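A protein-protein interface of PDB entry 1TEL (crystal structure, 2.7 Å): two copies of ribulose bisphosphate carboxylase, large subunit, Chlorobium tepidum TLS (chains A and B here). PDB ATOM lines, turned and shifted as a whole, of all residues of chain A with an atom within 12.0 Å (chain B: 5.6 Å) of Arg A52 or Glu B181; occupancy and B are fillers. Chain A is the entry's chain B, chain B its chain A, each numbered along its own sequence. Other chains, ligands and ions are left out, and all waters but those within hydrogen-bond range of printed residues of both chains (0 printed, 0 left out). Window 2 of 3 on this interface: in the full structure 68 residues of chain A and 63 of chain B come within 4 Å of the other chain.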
ATOM      1  N   ASP A   5     -36.507  26.978   7.292  1.00  0.00           N
ATOM      2  CA  ASP A   5     -35.273  27.089   8.057  1.00  0.00           C
ATOM      3  C   ASP A   5     -35.411  27.349   9.553  1.00  0.00           C
ATOM      4  O   ASP A   5     -34.634  26.808  10.335  1.00  0.00           O
ATOM      5  CB  ASP A   5     -34.389  28.167   7.444  1.00  0.00           C
ATOM      6  CG  ASP A   5     -34.082  27.900   5.987  1.00  0.00           C
ATOM      7  OD1 ASP A   5     -33.842  26.722   5.641  1.00  0.00           O
ATOM      8  OD2 ASP A   5     -34.073  28.866   5.193  1.00  0.00           O
ATOM      9  N   THR A  47     -24.068  29.622  12.977  1.00  0.00           N
ATOM     10  CA  THR A  47     -24.056  29.454  11.534  1.00  0.00           C
ATOM     11  C   THR A  47     -25.051  30.418  10.884  1.00  0.00           C
ATOM     12  O   THR A  47     -26.266  30.233  10.996  1.00  0.00           O
ATOM     13  CB  THR A  47     -24.415  27.995  11.148  1.00  0.00           C
ATOM     14  OG1 THR A  47     -25.718  27.669  11.644  1.00  0.00           O
ATOM     15  CG2 THR A  47     -23.399  27.019  11.747  1.00  0.00           C
ATOM     16  N   ALA A  48     -24.531  31.457  10.228  1.00  0.00           N
ATOM     17  CA  ALA A  48     -25.375  32.444   9.544  1.00  0.00           C
ATOM     18  C   ALA A  48     -25.820  31.843   8.212  1.00  0.00           C
ATOM     19  O   ALA A  48     -26.887  32.167   7.690  1.00  0.00           O
ATOM     20  CB  ALA A  48     -24.600  33.710   9.305  1.00  0.00           C
ATOM     21  N   GLN A  49     -24.968  30.973   7.670  1.00  0.00           N
ATOM     22  CA  GLN A  49     -25.216  30.252   6.426  1.00  0.00           C
ATOM     23  C   GLN A  49     -24.714  28.854   6.736  1.00  0.00           C
ATOM     24  O   GLN A  49     -23.553  28.668   7.099  1.00  0.00           O
ATOM     25  CB  GLN A  49     -24.428  30.869   5.268  1.00  0.00           C
ATOM     26  CG  GLN A  49     -24.913  32.263   4.898  1.00  0.00           C
ATOM     27  CD  GLN A  49     -24.155  32.877   3.731  1.00  0.00           C
ATOM     28  OE1 GLN A  49     -24.054  32.284   2.647  1.00  0.00           O
ATOM     29  NE2 GLN A  49     -23.626  34.081   3.943  1.00  0.00           N
ATOM     30  N   TRP A  50     -25.593  27.870   6.605  1.00  0.00           N
ATOM     31  CA  TRP A  50     -25.249  26.492   6.936  1.00  0.00           C
ATOM     32  C   TRP A  50     -25.037  25.551   5.769  1.00  0.00           C
ATOM     33  O   TRP A  50     -25.186  24.337   5.919  1.00  0.00           O
ATOM     34  CB  TRP A  50     -26.330  25.925   7.846  1.00  0.00           C
ATOM     35  CG  TRP A  50     -27.703  26.147   7.308  1.00  0.00           C
ATOM     36  CD1 TRP A  50     -28.447  25.275   6.575  1.00  0.00           C
ATOM     37  CD2 TRP A  50     -28.512  27.316   7.488  1.00  0.00           C
ATOM     38  NE1 TRP A  50     -29.677  25.820   6.296  1.00  0.00           N
ATOM     39  CE2 TRP A  50     -29.744  27.072   6.844  1.00  0.00           C
ATOM     40  CE3 TRP A  50     -28.314  28.546   8.135  1.00  0.00           C
ATOM     41  CZ2 TRP A  50     -30.781  28.009   6.828  1.00  0.00           C
ATOM     42  CZ3 TRP A  50     -29.347  29.482   8.116  1.00  0.00           C
ATOM     43  CH2 TRP A  50     -30.566  29.204   7.467  1.00  0.00           C
ATOM     44  N   LYS A  51     -24.690  26.105   4.615  1.00  0.00           N
ATOM     45  CA  LYS A  51     -24.451  25.300   3.421  1.00  0.00           C
ATOM     46  C   LYS A  51     -23.990  26.140   2.243  1.00  0.00           C
ATOM     47  O   LYS A  51     -24.258  27.340   2.175  1.00  0.00           O
ATOM     48  CB  LYS A  51     -25.723  24.558   2.995  1.00  0.00           C
ATOM     49  CG  LYS A  51     -26.810  25.464   2.423  1.00  0.00           C
ATOM     50  CD  LYS A  51     -27.789  24.660   1.597  1.00  0.00           C
ATOM     51  CE  LYS A  51     -28.399  23.545   2.429  1.00  0.00           C
ATOM     52  NZ  LYS A  51     -29.082  22.518   1.586  1.00  0.00           N
ATOM     53  N   ARG A  52     -23.289  25.498   1.315  1.00  0.00           N
ATOM     54  CA  ARG A  52     -22.839  26.181   0.110  1.00  0.00           C
ATOM     55  C   ARG A  52     -23.997  26.008  -0.864  1.00  0.00           C
ATOM     56  O   ARG A  52     -24.636  24.951  -0.896  1.00  0.00           O
ATOM     57  CB  ARG A  52     -21.559  25.536  -0.427  1.00  0.00           C
ATOM     58  CG  ARG A  52     -20.336  25.847   0.428  1.00  0.00           C
ATOM     59  CD  ARG A  52     -19.132  24.996   0.061  1.00  0.00           C
ATOM     60  NE  ARG A  52     -19.309  23.595   0.440  1.00  0.00           N
ATOM     61  CZ  ARG A  52     -18.390  22.651   0.260  1.00  0.00           C
ATOM     62  NH1 ARG A  52     -17.221  22.954  -0.297  1.00  0.00           N
ATOM     63  NH2 ARG A  52     -18.639  21.400   0.633  1.00  0.00           N
ATOM     64  N   VAL A  53     -24.292  27.047  -1.634  1.00  0.00           N
ATOM     65  CA  VAL A  53     -25.407  26.975  -2.571  1.00  0.00           C
ATOM     66  C   VAL A  53     -25.266  25.757  -3.482  1.00  0.00           C
ATOM     67  O   VAL A  53     -24.165  25.434  -3.945  1.00  0.00           O
ATOM     68  CB  VAL A  53     -25.512  28.259  -3.443  1.00  0.00           C
ATOM     69  CG1 VAL A  53     -26.875  28.305  -4.126  1.00  0.00           C
ATOM     70  CG2 VAL A  53     -25.305  29.509  -2.582  1.00  0.00           C
ATOM     71  N   GLY A  54     -26.386  25.076  -3.721  1.00  0.00           N
ATOM     72  CA  GLY A  54     -26.370  23.904  -4.574  1.00  0.00           C
ATOM     73  C   GLY A  54     -25.680  22.700  -3.962  1.00  0.00           C
ATOM     74  O   GLY A  54     -25.425  21.716  -4.652  1.00  0.00           O
ATOM     75  N   VAL A  55     -25.375  22.767  -2.670  1.00  0.00           N
ATOM     76  CA  VAL A  55     -24.718  21.653  -1.999  1.00  0.00           C
ATOM     77  C   VAL A  55     -25.625  21.024  -0.951  1.00  0.00           C
ATOM     78  O   VAL A  55     -26.327  21.723  -0.214  1.00  0.00           O
ATOM     79  CB  VAL A  55     -23.416  22.099  -1.321  1.00  0.00           C
ATOM     80  CG1 VAL A  55     -22.722  20.898  -0.694  1.00  0.00           C
ATOM     81  CG2 VAL A  55     -22.512  22.779  -2.339  1.00  0.00           C
ATOM     82  N   ASP A  56     -25.607  19.696  -0.895  1.00  0.00           N
ATOM     83  CA  ASP A  56     -26.427  18.954   0.057  1.00  0.00           C
ATOM     84  C   ASP A  56     -25.676  18.737   1.365  1.00  0.00           C
ATOM     85  O   ASP A  56     -25.042  17.693   1.576  1.00  0.00           O
ATOM     86  CB  ASP A  56     -26.838  17.603  -0.539  1.00  0.00           C
ATOM     87  CG  ASP A  56     -27.696  16.775   0.414  1.00  0.00           C
ATOM     88  OD1 ASP A  56     -27.147  16.233   1.404  1.00  0.00           O
ATOM     89  OD2 ASP A  56     -28.922  16.672   0.171  1.00  0.00           O
ATOM     90  N   GLU A  57     -25.749  19.732   2.240  1.00  0.00           N
ATOM     91  CA  GLU A  57     -25.077  19.665   3.527  1.00  0.00           C
ATOM     92  C   GLU A  57     -25.807  20.576   4.509  1.00  0.00           C
ATOM     93  O   GLU A  57     -26.583  21.444   4.092  1.00  0.00           O
ATOM     94  CB  GLU A  57     -23.620  20.109   3.371  1.00  0.00           C
ATOM     95  CG  GLU A  57     -23.445  21.582   3.032  1.00  0.00           C
ATOM     96  CD  GLU A  57     -22.030  21.926   2.617  1.00  0.00           C
ATOM     97  OE1 GLU A  57     -21.099  21.209   3.043  1.00  0.00           O
ATOM     98  OE2 GLU A  57     -21.848  22.919   1.874  1.00  0.00           O
ATOM     99  N   ASP A  58     -25.574  20.367   5.804  1.00  0.00           N
ATOM    100  CA  ASP A  58     -26.201  21.191   6.836  1.00  0.00           C
ATOM    101  C   ASP A  58     -25.287  21.331   8.050  1.00  0.00           C
ATOM    102  O   ASP A  58     -25.167  20.414   8.870  1.00  0.00           O
ATOM    103  CB  ASP A  58     -27.551  20.600   7.260  1.00  0.00           C
ATOM    104  CG  ASP A  58     -28.390  21.588   8.056  1.00  0.00           C
ATOM    105  OD1 ASP A  58     -29.575  21.290   8.334  1.00  0.00           O
ATOM    106  OD2 ASP A  58     -27.859  22.668   8.407  1.00  0.00           O
ATOM    107  N   PHE A  59     -24.647  22.492   8.166  1.00  0.00           N
ATOM    108  CA  PHE A  59     -23.724  22.745   9.270  1.00  0.00           C
ATOM    109  C   PHE A  59     -24.428  22.953  10.603  1.00  0.00           C
ATOM    110  O   PHE A  59     -23.805  22.858  11.663  1.00  0.00           O
ATOM    111  CB  PHE A  59     -22.849  23.972   8.968  1.00  0.00           C
ATOM    112  CG  PHE A  59     -22.161  23.922   7.625  1.00  0.00           C
ATOM    113  CD1 PHE A  59     -21.745  22.707   7.075  1.00  0.00           C
ATOM    114  CD2 PHE A  59     -21.904  25.095   6.921  1.00  0.00           C
ATOM    115  CE1 PHE A  59     -21.083  22.665   5.843  1.00  0.00           C
ATOM    116  CE2 PHE A  59     -21.244  25.064   5.693  1.00  0.00           C
ATOM    117  CZ  PHE A  59     -20.833  23.848   5.152  1.00  0.00           C
ATOM    118  N   ARG A  60     -25.730  23.222  10.541  1.00  0.00           N
ATOM    119  CA  ARG A  60     -26.525  23.468  11.736  1.00  0.00           C
ATOM    120  C   ARG A  60     -26.450  22.388  12.789  1.00  0.00           C
ATOM    121  O   ARG A  60     -26.259  22.676  13.965  1.00  0.00           O
ATOM    122  CB  ARG A  60     -27.980  23.718  11.357  1.00  0.00           C
ATOM    123  CG  ARG A  60     -28.173  25.088  10.757  1.00  0.00           C
ATOM    124  CD  ARG A  60     -29.613  25.367  10.437  1.00  0.00           C
ATOM    125  NE  ARG A  60     -30.130  24.435   9.449  1.00  0.00           N
ATOM    126  CZ  ARG A  60     -31.356  24.503   8.948  1.00  0.00           C
ATOM    127  NH1 ARG A  60     -32.179  25.460   9.348  1.00  0.00           N
ATOM    128  NH2 ARG A  60     -31.760  23.616   8.049  1.00  0.00           N
ATOM    129  N   VAL A  62     -24.188  20.338  13.845  1.00  0.00           N
ATOM    130  CA  VAL A  62     -23.078  20.376  14.795  1.00  0.00           C
ATOM    131  C   VAL A  62     -22.578  21.771  15.172  1.00  0.00           C
ATOM    132  O   VAL A  62     -21.969  21.941  16.237  1.00  0.00           O
ATOM    133  CB  VAL A  62     -21.864  19.535  14.295  1.00  0.00           C
ATOM    134  CG1 VAL A  62     -22.272  18.683  13.105  1.00  0.00           C
ATOM    135  CG2 VAL A  62     -20.701  20.442  13.936  1.00  0.00           C
ATOM    136  N   HIS A  63     -22.847  22.762  14.323  1.00  0.00           N
ATOM    137  CA  HIS A  63     -22.380  24.121  14.578  1.00  0.00           C
ATOM    138  C   HIS A  63     -23.430  25.191  14.883  1.00  0.00           C
ATOM    139  O   HIS A  63     -23.071  26.357  15.105  1.00  0.00           O
ATOM    140  CB  HIS A  63     -21.560  24.613  13.391  1.00  0.00           C
ATOM    141  CG  HIS A  63     -20.368  23.771  13.079  1.00  0.00           C
ATOM    142  ND1 HIS A  63     -19.306  23.637  13.943  1.00  0.00           N
ATOM    143  CD2 HIS A  63     -20.045  23.062  11.973  1.00  0.00           C
ATOM    144  CE1 HIS A  63     -18.376  22.887  13.382  1.00  0.00           C
ATOM    145  NE2 HIS A  63     -18.801  22.524  12.185  1.00  0.00           N
ATOM    146  N   PRO B 173     -19.863  30.391   3.295  1.00  0.00           N
ATOM    147  CA  PRO B 173     -20.156  30.115   4.707  1.00  0.00           C
ATOM    148  C   PRO B 173     -18.845  30.111   5.466  1.00  0.00           C
ATOM    149  O   PRO B 173     -17.793  29.850   4.885  1.00  0.00           O
ATOM    150  CB  PRO B 173     -20.776  28.718   4.680  1.00  0.00           C
ATOM    151  CG  PRO B 173     -21.191  28.523   3.250  1.00  0.00           C
ATOM    152  CD  PRO B 173     -20.109  29.193   2.478  1.00  0.00           C
ATOM    153  N   GLY B 176     -19.062  25.686   9.400  1.00  0.00           N
ATOM    154  CA  GLY B 176     -19.021  24.394   8.720  1.00  0.00           C
ATOM    155  C   GLY B 176     -17.929  24.028   7.706  1.00  0.00           C
ATOM    156  O   GLY B 176     -17.580  22.851   7.589  1.00  0.00           O
ATOM    157  N   LEU B 177     -17.399  25.005   6.967  1.00  0.00           N
ATOM    158  CA  LEU B 177     -16.368  24.734   5.965  1.00  0.00           C
ATOM    159  C   LEU B 177     -15.012  24.283   6.496  1.00  0.00           C
ATOM    160  O   LEU B 177     -14.642  24.552   7.640  1.00  0.00           O
ATOM    161  CB  LEU B 177     -16.158  25.953   5.064  1.00  0.00           C
ATOM    162  CG  LEU B 177     -17.278  26.298   4.079  1.00  0.00           C
ATOM    163  CD1 LEU B 177     -16.823  27.448   3.206  1.00  0.00           C
ATOM    164  CD2 LEU B 177     -17.621  25.094   3.219  1.00  0.00           C
ATOM    165  N   SER B 178     -14.274  23.600   5.631  1.00  0.00           N
ATOM    166  CA  SER B 178     -12.943  23.102   5.951  1.00  0.00           C
ATOM    167  C   SER B 178     -11.912  23.954   5.208  1.00  0.00           C
ATOM    168  O   SER B 178     -12.225  24.559   4.182  1.00  0.00           O
ATOM    169  CB  SER B 178     -12.803  21.651   5.498  1.00  0.00           C
ATOM    170  OG  SER B 178     -12.881  21.567   4.080  1.00  0.00           O
ATOM    171  N   PRO B 179     -10.663  23.995   5.710  1.00  0.00           N
ATOM    172  CA  PRO B 179      -9.578  24.769   5.098  1.00  0.00           C
ATOM    173  C   PRO B 179      -9.604  24.760   3.570  1.00  0.00           C
ATOM    174  O   PRO B 179      -9.588  25.812   2.934  1.00  0.00           O
ATOM    175  CB  PRO B 179      -8.337  24.106   5.671  1.00  0.00           C
ATOM    176  CG  PRO B 179      -8.781  23.810   7.085  1.00  0.00           C
ATOM    177  CD  PRO B 179     -10.165  23.229   6.873  1.00  0.00           C
ATOM    178  N   GLY B 180      -9.657  23.569   2.987  1.00  0.00           N
ATOM    179  CA  GLY B 180      -9.694  23.464   1.543  1.00  0.00           C
ATOM    180  C   GLY B 180     -10.923  24.113   0.932  1.00  0.00           C
ATOM    181  O   GLY B 180     -10.803  24.952   0.036  1.00  0.00           O
ATOM    182  N   GLU B 181     -12.106  23.731   1.412  1.00  0.00           N
ATOM    183  CA  GLU B 181     -13.358  24.280   0.896  1.00  0.00           C
ATOM    184  C   GLU B 181     -13.386  25.798   1.022  1.00  0.00           C
ATOM    185  O   GLU B 181     -13.755  26.511   0.088  1.00  0.00           O
ATOM    186  CB  GLU B 181     -14.541  23.674   1.653  1.00  0.00           C
ATOM    187  CG  GLU B 181     -14.610  22.159   1.556  1.00  0.00           C
ATOM    188  CD  GLU B 181     -15.621  21.553   2.510  1.00  0.00           C
ATOM    189  OE1 GLU B 181     -15.889  20.339   2.403  1.00  0.00           O
ATOM    190  OE2 GLU B 181     -16.150  22.287   3.374  1.00  0.00           O
ATOM    191  N   PHE B 182     -12.981  26.275   2.191  1.00  0.00           N
ATOM    192  CA  PHE B 182     -12.927  27.692   2.505  1.00  0.00           C
ATOM    193  C   PHE B 182     -12.003  28.408   1.526  1.00  0.00           C
ATOM    194  O   PHE B 182     -12.345  29.459   0.977  1.00  0.00           O
ATOM    195  CB  PHE B 182     -12.421  27.839   3.937  1.00  0.00           C
ATOM    196  CG  PHE B 182     -12.422  29.242   4.458  1.00  0.00           C
ATOM    197  CD1 PHE B 182     -11.364  30.089   4.207  1.00  0.00           C
ATOM    198  CD2 PHE B 182     -13.459  29.690   5.264  1.00  0.00           C
ATOM    199  CE1 PHE B 182     -11.326  31.364   4.760  1.00  0.00           C
ATOM    200  CE2 PHE B 182     -13.436  30.966   5.825  1.00  0.00           C
ATOM    201  CZ  PHE B 182     -12.365  31.803   5.573  1.00  0.00           C
ATOM    202  N   ALA B 183     -10.840  27.815   1.291  1.00  0.00           N
ATOM    203  CA  ALA B 183      -9.850  28.387   0.384  1.00  0.00           C
ATOM    204  C   ALA B 183     -10.308  28.649  -1.051  1.00  0.00           C
ATOM    205  O   ALA B 183      -9.862  29.606  -1.669  1.00  0.00           O
ATOM    206  CB  ALA B 183      -8.608  27.507   0.367  1.00  0.00           C
ATOM    207  N   GLU B 184     -11.185  27.810  -1.590  1.00  0.00           N
ATOM    208  CA  GLU B 184     -11.635  27.985  -2.970  1.00  0.00           C
ATOM    209  C   GLU B 184     -12.542  29.195  -3.102  1.00  0.00           C
ATOM    210  O   GLU B 184     -12.471  29.929  -4.092  1.00  0.00           O
ATOM    211  CB  GLU B 184     -12.372  26.734  -3.471  1.00  0.00           C
ATOM    212  CG  GLU B 184     -11.934  26.237  -4.871  1.00  0.00           C
ATOM    213  CD  GLU B 184     -12.103  27.278  -5.998  1.00  0.00           C
ATOM    214  OE1 GLU B 184     -11.262  28.202  -6.107  1.00  0.00           O
ATOM    215  OE2 GLU B 184     -13.082  27.174  -6.780  1.00  0.00           O
ATOM    216  N   ILE B 185     -13.391  29.414  -2.103  1.00  0.00           N
ATOM    217  CA  ILE B 185     -14.294  30.550  -2.150  1.00  0.00           C
ATOM    218  C   ILE B 185     -13.510  31.856  -2.016  1.00  0.00           C
ATOM    219  O   ILE B 185     -13.788  32.831  -2.716  1.00  0.00           O
ATOM    220  CB  ILE B 185     -15.360  30.435  -1.055  1.00  0.00           C
ATOM    221  CG1 ILE B 185     -16.075  29.087  -1.188  1.00  0.00           C
ATOM    222  CG2 ILE B 185     -16.358  31.560  -1.192  1.00  0.00           C
ATOM    223  CD1 ILE B 185     -17.138  28.809  -0.130  1.00  0.00           C
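The backbone carbonyl oxygen of Trp A50 is in hydrogen-bond range of the backbone NH of Phe A59, 3.0 Å away.
The guanidinium group (NE) of Arg A52 is in salt-bridge range of the side-chain carboxylate (OE2) of Glu A57 (3.0 Å).
OE2 of Glu B181 lies within hydrogen-bond range of N of Ser B178 (3.2 Å).
The backbone carbonyl oxygen (O) of Val A55 is in hydrogen-bond range of the side-chain amino group (NZ) of Lys A51 (3.4 Å).
Asp A5 touches none of the printed residues of chain B.
Of the printed residues of chain B, Gln A49 touches Pro B173 (3.7 Å).
Printed residues of chain B within 4 Å of Lys A51: Pro B173 (3.5 Å).
Of the printed residues of chain B, Arg A52 touches Pro B173 (3.9 Å), Leu B177 (3.5 Å) and Glu B181 (3.3 Å).
Printed residues of chain B within 4 Å of Phe A59: Pro B173 (3.8 Å), Gly B176 (3.4 Å) and Leu B177 (3.95 Å).
Printed residues of chain B within 4 Å of His A63: Gly B176.
Of the printed residues of chain A, Pro B173 touches Gln A49, Lys A51, Arg A52 and Phe A59.
Gly B176 touches just these residues of chain A: Phe A59 (3.4 Å) and His A63 (3.7 Å).
Leu B177 touches just these residues of chain A: Arg A52 (3.5 Å) and Phe A59 (3.95 Å).
No residue of chain A comes within 4 Å of Ser B178.
Pro B179 touches none of the printed residues of chain A.
No residue of chain A comes within 4 Å of Gly B180.
No residue of chain A comes within 4 Å of Phe B182.
No residue of chain A comes within 4 Å of Glu B184.
No residue of chain A comes within 4 Å of Ile B185.
The nearest residue of chain A that does not touch Glu B181 is Glu A57 (5.1 Å).
The nearest printed residue of chain B that does not touch His A63 is Leu B177 (5.9 Å).
Of the 17 printed residues of chain A, 5 touch a printed residue of chain B.
Printed residues of chain A that touch a printed residue of chain B: Gln A49, Lys A51, Arg A52, Phe A59 and His A63.
Hydrophobic or aromatic side chains of chain B that line the printed part of chain A: Pro B173 and Leu B177.
Among the printed residues, Asp or Glu carboxylates within 4 Å of a Lys or Arg side-chain nitrogen of the other chain: Arg A52 with Glu B181.
OE1 of Glu B181 is in salt-bridge range of NH2 of Arg A52, 3.4 Å away.
No position is printed for both chains.
Among the printed residues, merely in contact across the chains: Phe A59 with Gly B176 (3.4 Å), Lys A51 with Pro B173 (3.5 Å), Arg A52 with Leu B177 (3.5 Å), His A63 with Gly B176 (3.7 Å), Gln A49 with Pro B173 (3.7 Å), Phe A59 with Pro B173 (3.8 Å), Arg A52 with Pro B173 (3.9 Å) and Phe A59 with Leu B177 (3.95 Å).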
